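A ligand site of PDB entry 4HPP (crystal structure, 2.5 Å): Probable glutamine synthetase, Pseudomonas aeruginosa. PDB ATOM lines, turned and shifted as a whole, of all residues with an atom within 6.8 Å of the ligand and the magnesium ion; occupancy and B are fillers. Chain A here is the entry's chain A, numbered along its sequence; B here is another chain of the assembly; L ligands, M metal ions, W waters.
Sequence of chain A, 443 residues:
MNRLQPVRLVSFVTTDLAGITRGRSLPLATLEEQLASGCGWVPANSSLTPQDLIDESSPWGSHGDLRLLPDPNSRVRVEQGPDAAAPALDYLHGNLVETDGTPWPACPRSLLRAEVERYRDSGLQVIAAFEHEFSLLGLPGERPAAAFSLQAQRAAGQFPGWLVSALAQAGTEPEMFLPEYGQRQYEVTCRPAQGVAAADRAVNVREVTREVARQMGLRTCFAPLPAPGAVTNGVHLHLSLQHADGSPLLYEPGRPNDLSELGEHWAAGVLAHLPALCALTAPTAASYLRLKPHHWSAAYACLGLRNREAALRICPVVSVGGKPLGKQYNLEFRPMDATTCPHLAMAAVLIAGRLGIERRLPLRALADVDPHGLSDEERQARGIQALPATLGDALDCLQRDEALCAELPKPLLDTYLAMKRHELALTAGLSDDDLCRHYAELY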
ATOM      1  N   GLU A 131     -23.528  -4.574 -21.546  1.00  0.00           N
ATOM      2  CA  GLU A 131     -22.118  -4.297 -21.382  1.00  0.00           C
ATOM      3  C   GLU A 131     -21.605  -4.131 -22.784  1.00  0.00           C
ATOM      4  O   GLU A 131     -21.943  -4.949 -23.654  1.00  0.00           O
ATOM      5  CB  GLU A 131     -21.379  -5.460 -20.706  1.00  0.00           C
ATOM      6  CG  GLU A 131     -21.680  -5.742 -19.219  1.00  0.00           C
ATOM      7  CD  GLU A 131     -20.784  -6.858 -18.628  1.00  0.00           C
ATOM      8  OE1 GLU A 131     -20.778  -6.986 -17.386  1.00  0.00           O
ATOM      9  OE2 GLU A 131     -20.049  -7.600 -19.368  1.00  0.00           O
ATOM     10  N   HIS A 132     -20.790  -3.108 -22.993  1.00  0.00           N
ATOM     11  CA  HIS A 132     -20.349  -2.733 -24.304  1.00  0.00           C
ATOM     12  C   HIS A 132     -18.861  -2.739 -24.423  1.00  0.00           C
ATOM     13  O   HIS A 132     -18.171  -2.208 -23.546  1.00  0.00           O
ATOM     14  CB  HIS A 132     -20.874  -1.359 -24.624  1.00  0.00           C
ATOM     15  CG  HIS A 132     -22.382  -1.319 -24.894  1.00  0.00           C
ATOM     16  ND1 HIS A 132     -23.265  -0.755 -24.019  1.00  0.00           N
ATOM     17  CD2 HIS A 132     -23.122  -1.700 -26.022  1.00  0.00           C
ATOM     18  CE1 HIS A 132     -24.507  -0.805 -24.555  1.00  0.00           C
ATOM     19  NE2 HIS A 132     -24.412  -1.391 -25.765  1.00  0.00           N
ATOM     20  N   GLU A 133     -18.346  -3.367 -25.501  1.00  0.00           N
ATOM     21  CA  GLU A 133     -16.930  -3.305 -25.767  1.00  0.00           C
ATOM     22  C   GLU A 133     -16.698  -2.550 -27.107  1.00  0.00           C
ATOM     23  O   GLU A 133     -17.531  -2.594 -28.024  1.00  0.00           O
ATOM     24  CB  GLU A 133     -16.306  -4.681 -25.771  1.00  0.00           C
ATOM     25  CG  GLU A 133     -16.182  -5.332 -24.395  1.00  0.00           C
ATOM     26  CD  GLU A 133     -15.937  -6.835 -24.495  1.00  0.00           C
ATOM     27  OE1 GLU A 133     -16.076  -7.413 -25.614  1.00  0.00           O
ATOM     28  OE2 GLU A 133     -15.626  -7.459 -23.427  1.00  0.00           O
ATOM     29  N   PHE A 148      -5.652  -5.497 -20.631  1.00  0.00           N
ATOM     30  CA  PHE A 148      -6.169  -5.338 -19.260  1.00  0.00           C
ATOM     31  C   PHE A 148      -5.297  -4.417 -18.369  1.00  0.00           C
ATOM     32  O   PHE A 148      -5.525  -4.337 -17.184  1.00  0.00           O
ATOM     33  CB  PHE A 148      -6.322  -6.736 -18.582  1.00  0.00           C
ATOM     34  CG  PHE A 148      -7.236  -7.728 -19.295  1.00  0.00           C
ATOM     35  CD1 PHE A 148      -6.958  -9.088 -19.235  1.00  0.00           C
ATOM     36  CD2 PHE A 148      -8.384  -7.333 -19.961  1.00  0.00           C
ATOM     37  CE1 PHE A 148      -7.785 -10.032 -19.867  1.00  0.00           C
ATOM     38  CE2 PHE A 148      -9.194  -8.269 -20.604  1.00  0.00           C
ATOM     39  CZ  PHE A 148      -8.896  -9.610 -20.564  1.00  0.00           C
ATOM     40  N   LEU A 178     -12.743  -0.004 -18.278  1.00  0.00           N
ATOM     41  CA  LEU A 178     -11.563  -0.865 -18.200  1.00  0.00           C
ATOM     42  C   LEU A 178     -10.968  -1.125 -19.581  1.00  0.00           C
ATOM     43  O   LEU A 178     -11.714  -1.246 -20.549  1.00  0.00           O
ATOM     44  CB  LEU A 178     -11.962  -2.189 -17.511  1.00  0.00           C
ATOM     45  CG  LEU A 178     -13.184  -2.999 -18.004  1.00  0.00           C
ATOM     46  CD1 LEU A 178     -12.749  -4.245 -18.764  1.00  0.00           C
ATOM     47  CD2 LEU A 178     -14.107  -3.393 -16.859  1.00  0.00           C
ATOM     48  N   GLU A 180      -9.707  -3.728 -22.247  1.00  0.00           N
ATOM     49  CA  GLU A 180     -10.092  -5.138 -22.409  1.00  0.00           C
ATOM     50  C   GLU A 180      -8.974  -5.948 -23.146  1.00  0.00           C
ATOM     51  O   GLU A 180      -7.818  -5.496 -23.286  1.00  0.00           O
ATOM     52  CB  GLU A 180     -11.391  -5.232 -23.213  1.00  0.00           C
ATOM     53  CG  GLU A 180     -12.622  -5.564 -22.392  1.00  0.00           C
ATOM     54  CD  GLU A 180     -12.766  -7.034 -22.052  1.00  0.00           C
ATOM     55  OE1 GLU A 180     -13.732  -7.388 -21.363  1.00  0.00           O
ATOM     56  OE2 GLU A 180     -11.920  -7.841 -22.486  1.00  0.00           O
ATOM     57  N   TYR A 181      -9.348  -7.110 -23.671  1.00  0.00           N
ATOM     58  CA  TYR A 181      -8.348  -8.079 -24.144  1.00  0.00           C
ATOM     59  C   TYR A 181      -7.661  -7.602 -25.424  1.00  0.00           C
ATOM     60  O   TYR A 181      -6.442  -7.671 -25.521  1.00  0.00           O
ATOM     61  CB  TYR A 181      -8.918  -9.560 -24.149  1.00  0.00           C
ATOM     62  CG  TYR A 181      -7.928 -10.605 -24.557  1.00  0.00           C
ATOM     63  CD1 TYR A 181      -6.663 -10.677 -23.946  1.00  0.00           C
ATOM     64  CD2 TYR A 181      -8.240 -11.523 -25.578  1.00  0.00           C
ATOM     65  CE1 TYR A 181      -5.727 -11.617 -24.349  1.00  0.00           C
ATOM     66  CE2 TYR A 181      -7.307 -12.463 -25.995  1.00  0.00           C
ATOM     67  CZ  TYR A 181      -6.063 -12.516 -25.396  1.00  0.00           C
ATOM     68  OH  TYR A 181      -5.160 -13.455 -25.813  1.00  0.00           O
ATOM     69  N   GLN A 185      -8.878  -2.069 -27.141  1.00  0.00           N
ATOM     70  CA  GLN A 185     -10.203  -2.377 -26.707  1.00  0.00           C
ATOM     71  C   GLN A 185     -10.457  -1.846 -25.288  1.00  0.00           C
ATOM     72  O   GLN A 185      -9.601  -2.021 -24.370  1.00  0.00           O
ATOM     73  CB  GLN A 185     -10.417  -3.861 -26.742  1.00  0.00           C
ATOM     74  CG  GLN A 185     -11.896  -4.217 -26.707  1.00  0.00           C
ATOM     75  CD  GLN A 185     -12.172  -5.702 -26.714  1.00  0.00           C
ATOM     76  OE1 GLN A 185     -11.383  -6.513 -26.197  1.00  0.00           O
ATOM     77  NE2 GLN A 185     -13.324  -6.068 -27.281  1.00  0.00           N
ATOM     78  N   GLU A 187     -13.980  -1.269 -22.321  1.00  0.00           N
ATOM     79  CA  GLU A 187     -15.326  -1.627 -21.937  1.00  0.00           C
ATOM     80  C   GLU A 187     -15.834  -0.656 -20.887  1.00  0.00           C
ATOM     81  O   GLU A 187     -15.158  -0.321 -19.910  1.00  0.00           O
ATOM     82  CB  GLU A 187     -15.371  -3.051 -21.418  1.00  0.00           C
ATOM     83  CG  GLU A 187     -16.800  -3.571 -21.239  1.00  0.00           C
ATOM     84  CD  GLU A 187     -16.888  -4.949 -20.561  1.00  0.00           C
ATOM     85  OE1 GLU A 187     -18.007  -5.433 -20.290  1.00  0.00           O
ATOM     86  OE2 GLU A 187     -15.846  -5.566 -20.302  1.00  0.00           O
ATOM     87  N   PRO A 224     -18.749  -6.048 -34.506  1.00  0.00           N
ATOM     88  CA  PRO A 224     -18.363  -7.297 -33.839  1.00  0.00           C
ATOM     89  C   PRO A 224     -16.890  -7.639 -34.045  1.00  0.00           C
ATOM     90  O   PRO A 224     -16.241  -8.071 -33.078  1.00  0.00           O
ATOM     91  CB  PRO A 224     -19.303  -8.371 -34.462  1.00  0.00           C
ATOM     92  CG  PRO A 224     -20.379  -7.631 -35.169  1.00  0.00           C
ATOM     93  CD  PRO A 224     -19.962  -6.179 -35.326  1.00  0.00           C
ATOM     94  N   VAL A 231      -9.250  -9.481 -31.546  1.00  0.00           N
ATOM     95  CA  VAL A 231     -10.270  -9.746 -30.526  1.00  0.00           C
ATOM     96  C   VAL A 231     -11.587  -9.031 -30.856  1.00  0.00           C
ATOM     97  O   VAL A 231     -11.593  -7.874 -31.293  1.00  0.00           O
ATOM     98  CB  VAL A 231      -9.785  -9.285 -29.132  1.00  0.00           C
ATOM     99  CG1 VAL A 231     -10.734  -9.782 -28.028  1.00  0.00           C
ATOM    100  CG2 VAL A 231      -8.333  -9.787 -28.913  1.00  0.00           C
ATOM    101  N   THR A 232     -12.688  -9.754 -30.677  1.00  0.00           N
ATOM    102  CA  THR A 232     -14.007  -9.363 -31.098  1.00  0.00           C
ATOM    103  C   THR A 232     -14.643  -8.453 -30.018  1.00  0.00           C
ATOM    104  O   THR A 232     -14.238  -8.509 -28.855  1.00  0.00           O
ATOM    105  CB  THR A 232     -14.909 -10.608 -31.329  1.00  0.00           C
ATOM    106  OG1 THR A 232     -14.740 -11.558 -30.265  1.00  0.00           O
ATOM    107  CG2 THR A 232     -14.552 -11.336 -32.571  1.00  0.00           C
ATOM    108  N   ASN A 233     -15.633  -7.629 -30.408  1.00  0.00           N
ATOM    109  CA  ASN A 233     -16.323  -6.692 -29.542  1.00  0.00           C
ATOM    110  C   ASN A 233     -17.709  -7.327 -29.287  1.00  0.00           C
ATOM    111  O   ASN A 233     -18.574  -7.380 -30.197  1.00  0.00           O
ATOM    112  CB  ASN A 233     -16.476  -5.279 -30.165  1.00  0.00           C
ATOM    113  CG  ASN A 233     -15.152  -4.487 -30.365  1.00  0.00           C
ATOM    114  OD1 ASN A 233     -14.320  -4.350 -29.438  1.00  0.00           O
ATOM    115  ND2 ASN A 233     -14.966  -3.921 -31.598  1.00  0.00           N
ATOM    116  N   GLY A 234     -17.923  -7.821 -28.066  1.00  0.00           N
ATOM    117  CA  GLY A 234     -19.215  -8.352 -27.663  1.00  0.00           C
ATOM    118  C   GLY A 234     -20.112  -7.302 -27.035  1.00  0.00           C
ATOM    119  O   GLY A 234     -19.680  -6.186 -26.780  1.00  0.00           O
ATOM    120  N   VAL A 235     -21.376  -7.656 -26.857  1.00  0.00           N
ATOM    121  CA  VAL A 235     -22.335  -6.929 -26.069  1.00  0.00           C
ATOM    122  C   VAL A 235     -22.924  -8.045 -25.207  1.00  0.00           C
ATOM    123  O   VAL A 235     -23.267  -9.076 -25.725  1.00  0.00           O
ATOM    124  CB  VAL A 235     -23.438  -6.278 -26.932  1.00  0.00           C
ATOM    125  CG1 VAL A 235     -24.692  -5.937 -26.091  1.00  0.00           C
ATOM    126  CG2 VAL A 235     -22.940  -5.017 -27.623  1.00  0.00           C
ATOM    127  N   HIS A 236     -23.028  -7.842 -23.903  1.00  0.00           N
ATOM    128  CA  HIS A 236     -23.634  -8.850 -23.037  1.00  0.00           C
ATOM    129  C   HIS A 236     -24.773  -8.258 -22.306  1.00  0.00           C
ATOM    130  O   HIS A 236     -24.689  -7.179 -21.752  1.00  0.00           O
ATOM    131  CB  HIS A 236     -22.648  -9.418 -22.009  1.00  0.00           C
ATOM    132  CG  HIS A 236     -21.468 -10.123 -22.612  1.00  0.00           C
ATOM    133  ND1 HIS A 236     -20.288 -10.240 -21.953  1.00  0.00           N
ATOM    134  CD2 HIS A 236     -21.280 -10.745 -23.861  1.00  0.00           C
ATOM    135  CE1 HIS A 236     -19.389 -10.905 -22.746  1.00  0.00           C
ATOM    136  NE2 HIS A 236     -19.992 -11.206 -23.914  1.00  0.00           N
ATOM    137  N   ARG A 290     -17.612 -13.223 -35.583  1.00  0.00           N
ATOM    138  CA  ARG A 290     -17.513 -13.222 -34.107  1.00  0.00           C
ATOM    139  C   ARG A 290     -18.095 -14.513 -33.469  1.00  0.00           C
ATOM    140  O   ARG A 290     -17.426 -15.179 -32.624  1.00  0.00           O
ATOM    141  CB  ARG A 290     -18.146 -11.941 -33.510  1.00  0.00           C
ATOM    142  CG  ARG A 290     -18.501 -12.051 -32.043  1.00  0.00           C
ATOM    143  CD  ARG A 290     -18.892 -10.702 -31.392  1.00  0.00           C
ATOM    144  NE  ARG A 290     -19.043 -10.938 -29.967  1.00  0.00           N
ATOM    145  CZ  ARG A 290     -20.121 -11.466 -29.369  1.00  0.00           C
ATOM    146  NH1 ARG A 290     -20.099 -11.666 -28.054  1.00  0.00           N
ATOM    147  NH2 ARG A 290     -21.221 -11.753 -30.037  1.00  0.00           N
ATOM    148  N   ARG A 308     -17.398 -19.357 -20.027  1.00  0.00           N
ATOM    149  CA  ARG A 308     -17.876 -18.438 -21.055  1.00  0.00           C
ATOM    150  C   ARG A 308     -17.646 -19.013 -22.453  1.00  0.00           C
ATOM    151  O   ARG A 308     -17.237 -18.334 -23.383  1.00  0.00           O
ATOM    152  CB  ARG A 308     -17.176 -17.088 -20.911  1.00  0.00           C
ATOM    153  CG  ARG A 308     -17.333 -16.482 -19.544  1.00  0.00           C
ATOM    154  CD  ARG A 308     -16.261 -15.442 -19.287  1.00  0.00           C
ATOM    155  NE  ARG A 308     -16.210 -15.146 -17.853  1.00  0.00           N
ATOM    156  CZ  ARG A 308     -15.866 -13.981 -17.329  1.00  0.00           C
ATOM    157  NH1 ARG A 308     -15.529 -12.941 -18.097  1.00  0.00           N
ATOM    158  NH2 ARG A 308     -15.855 -13.850 -16.000  1.00  0.00           N
ATOM    159  N   GLU A 332     -26.815 -13.730 -17.916  1.00  0.00           N
ATOM    160  CA  GLU A 332     -26.136 -13.079 -18.974  1.00  0.00           C
ATOM    161  C   GLU A 332     -26.184 -13.873 -20.302  1.00  0.00           C
ATOM    162  O   GLU A 332     -25.639 -14.994 -20.397  1.00  0.00           O
ATOM    163  CB  GLU A 332     -24.697 -12.901 -18.514  1.00  0.00           C
ATOM    164  CG  GLU A 332     -23.679 -12.866 -19.615  1.00  0.00           C
ATOM    165  CD  GLU A 332     -22.406 -12.180 -19.206  1.00  0.00           C
ATOM    166  OE1 GLU A 332     -22.398 -10.940 -19.015  1.00  0.00           O
ATOM    167  OE2 GLU A 332     -21.394 -12.881 -19.095  1.00  0.00           O
ATOM    168  N   ARG A 334     -25.045 -13.914 -24.295  1.00  0.00           N
ATOM    169  CA  ARG A 334     -23.708 -13.576 -24.733  1.00  0.00           C
ATOM    170  C   ARG A 334     -23.574 -13.449 -26.243  1.00  0.00           C
ATOM    171  O   ARG A 334     -22.687 -12.691 -26.698  1.00  0.00           O
ATOM    172  CB  ARG A 334     -22.650 -14.526 -24.156  1.00  0.00           C
ATOM    173  CG  ARG A 334     -22.700 -14.595 -22.652  1.00  0.00           C
ATOM    174  CD  ARG A 334     -21.585 -15.396 -22.015  1.00  0.00           C
ATOM    175  NE  ARG A 334     -20.393 -14.580 -21.777  1.00  0.00           N
ATOM    176  CZ  ARG A 334     -19.258 -14.746 -22.444  1.00  0.00           C
ATOM    177  NH1 ARG A 334     -18.196 -13.963 -22.184  1.00  0.00           N
ATOM    178  NH2 ARG A 334     -19.196 -15.713 -23.373  1.00  0.00           N
ATOM    179  N   MET A 336     -24.377 -11.613 -28.576  1.00  0.00           N
ATOM    180  CA  MET A 336     -24.969 -10.328 -28.885  1.00  0.00           C
ATOM    181  C   MET A 336     -23.838  -9.383 -29.176  1.00  0.00           C
ATOM    182  O   MET A 336     -22.749  -9.567 -28.625  1.00  0.00           O
ATOM    183  CB  MET A 336     -25.830  -9.847 -27.742  1.00  0.00           C
ATOM    184  CG  MET A 336     -26.647  -8.647 -28.152  1.00  0.00           C
ATOM    185  SD  MET A 336     -27.616  -7.946 -26.797  1.00  0.00           S
ATOM    186  CE  MET A 336     -29.129  -8.977 -26.790  1.00  0.00           C
ATOM    187  N   VAL B  42     -10.701 -12.624 -13.876  1.00  0.00           N
ATOM    188  CA  VAL B  42     -10.889 -13.942 -14.562  1.00  0.00           C
ATOM    189  C   VAL B  42      -9.603 -14.736 -14.264  1.00  0.00           C
ATOM    190  O   VAL B  42      -8.513 -14.220 -14.481  1.00  0.00           O
ATOM    191  CB  VAL B  42     -11.154 -13.732 -16.080  1.00  0.00           C
ATOM    192  CG1 VAL B  42     -11.081 -15.020 -16.886  1.00  0.00           C
ATOM    193  CG2 VAL B  42     -12.503 -13.042 -16.302  1.00  0.00           C
HETATM  194  N1  LIG L   1     -14.821  -9.771 -26.331  1.00  0.00           N
HETATM  195  C1  LIG L   1     -15.710 -10.951 -25.947  1.00  0.00           C
HETATM  196  C2  LIG L   1     -17.016 -11.098 -26.754  1.00  0.00           C
HETATM  197  O1  LIG L   1     -17.036 -10.966 -27.979  1.00  0.00           O
HETATM  198  C3  LIG L   1     -16.048 -10.895 -24.463  1.00  0.00           C
HETATM  199  C4  LIG L   1     -14.869 -11.186 -23.570  1.00  0.00           C
HETATM  200  C5  LIG L   1     -15.173 -10.911 -22.141  1.00  0.00           C
HETATM  201  O2  LIG L   1     -15.195 -11.888 -21.376  1.00  0.00           O
HETATM  202  O3  LIG L   1     -15.410  -9.732 -21.773  1.00  0.00           O
HETATM  203  O4  LIG L   1     -18.103 -11.350 -26.220  1.00  0.00           O
HETATM  204 MG    MG M   1     -15.823  -7.874 -21.310  1.00  0.00          MG
HETATM  205  O   HOH W   1     -18.876  -7.712 -22.294  1.00  0.00           O
HETATM  206  O   HOH W   2     -12.299  -9.028 -25.337  1.00  0.00           O
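A nitrogen (N1) of the ligand sits at hydrogen-bond distance from the backbone carbonyl oxygen (O) of Thr 232 (2.9 Å).
O4 of the ligand lies within hydrogen-bond range of NE2 of His 236, at 3.0 Å.
The guanidinium group (NH1) of Arg 334 is in salt-bridge range of an oxygen (O2) of the ligand (3.7 Å).
The backbone NH (N) of Gly 234 lies within hydrogen-bond range of an oxygen (O1) of the ligand (3.3 Å).
NH1 of Arg 308 lies within salt-bridge range of O2 of the ligand (3.5 Å).
O4 of the ligand is in salt-bridge range of NH1 of Arg 290 (2.7 Å).
OG1 of Thr 232 sits at hydrogen-bond distance from O1 of the ligand, 3.3 Å away.
NH1 of Arg 290 is in hydrogen-bond range of O of Arg 334 (3.1 Å).
N of Glu 180 sits at hydrogen-bond distance from O of Gln 185 (2.7 Å).
The backbone carbonyl oxygen (O) of Leu 178 sits at hydrogen-bond distance from the backbone NH (N) of Glu 187 (2.9 Å).
The guanidinium group of Arg 290 sits at hydrogen-bond distance from the backbone carbonyl oxygen of Met 336.
The backbone NH (N) of Asn 233 lies within hydrogen-bond range of the backbone carbonyl oxygen (O) of Pro 224 (2.8 Å).
The side-chain amide oxygen of Asn 233 sits at hydrogen-bond distance from the side-chain amide nitrogen of Gln 185, 2.9 Å away.
OE1 of Glu 133 sits at hydrogen-bond distance from N of Gly 234.
The guanidinium group of Arg 334 is in salt-bridge range of the side-chain carboxylate of Glu 332, at 3.3 Å.
Merely in contact with the ligand: Asn 233 (3.9 Å).
Hydrophobic or aromatic side chains that line the ligand: His 236.
Within 4 Å of the ligand: Glu 133, Glu 180, Thr 232, Asn 233, Gly 234, His 236, Arg 290, Arg 308 and Arg 334.
The nearest printed residue that does not touch the ligand is Gln 185 (4.1 Å).
Three residues have an atom within 4 Å of the magnesium ion: Glu 133, Glu 180 and Glu 187.
The magnesium ion is bound by an oxygen (O3) of the ligand (2.0 Å), the side-chain carboxylate (OE1) of Glu 180 (2.1 Å), the side-chain carboxylate (OE2) of Glu 133 (2.2 Å) and the side-chain carboxylate (OE2) of Glu 187 (2.5 Å).
Water W2 lies within hydrogen-bond range of a nitrogen (N1) of the ligand (2.8 Å), the side-chain amide oxygen of Gln 185 (2.8 Å) and the side-chain carboxylate of Glu 180 (3.1 Å).
Water W1 lies within hydrogen-bond range of a ring nitrogen (ND1) of His 236, the side-chain carboxylate (OE2) of Glu 131 and the side-chain carboxylate (OE1) of Glu 187.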
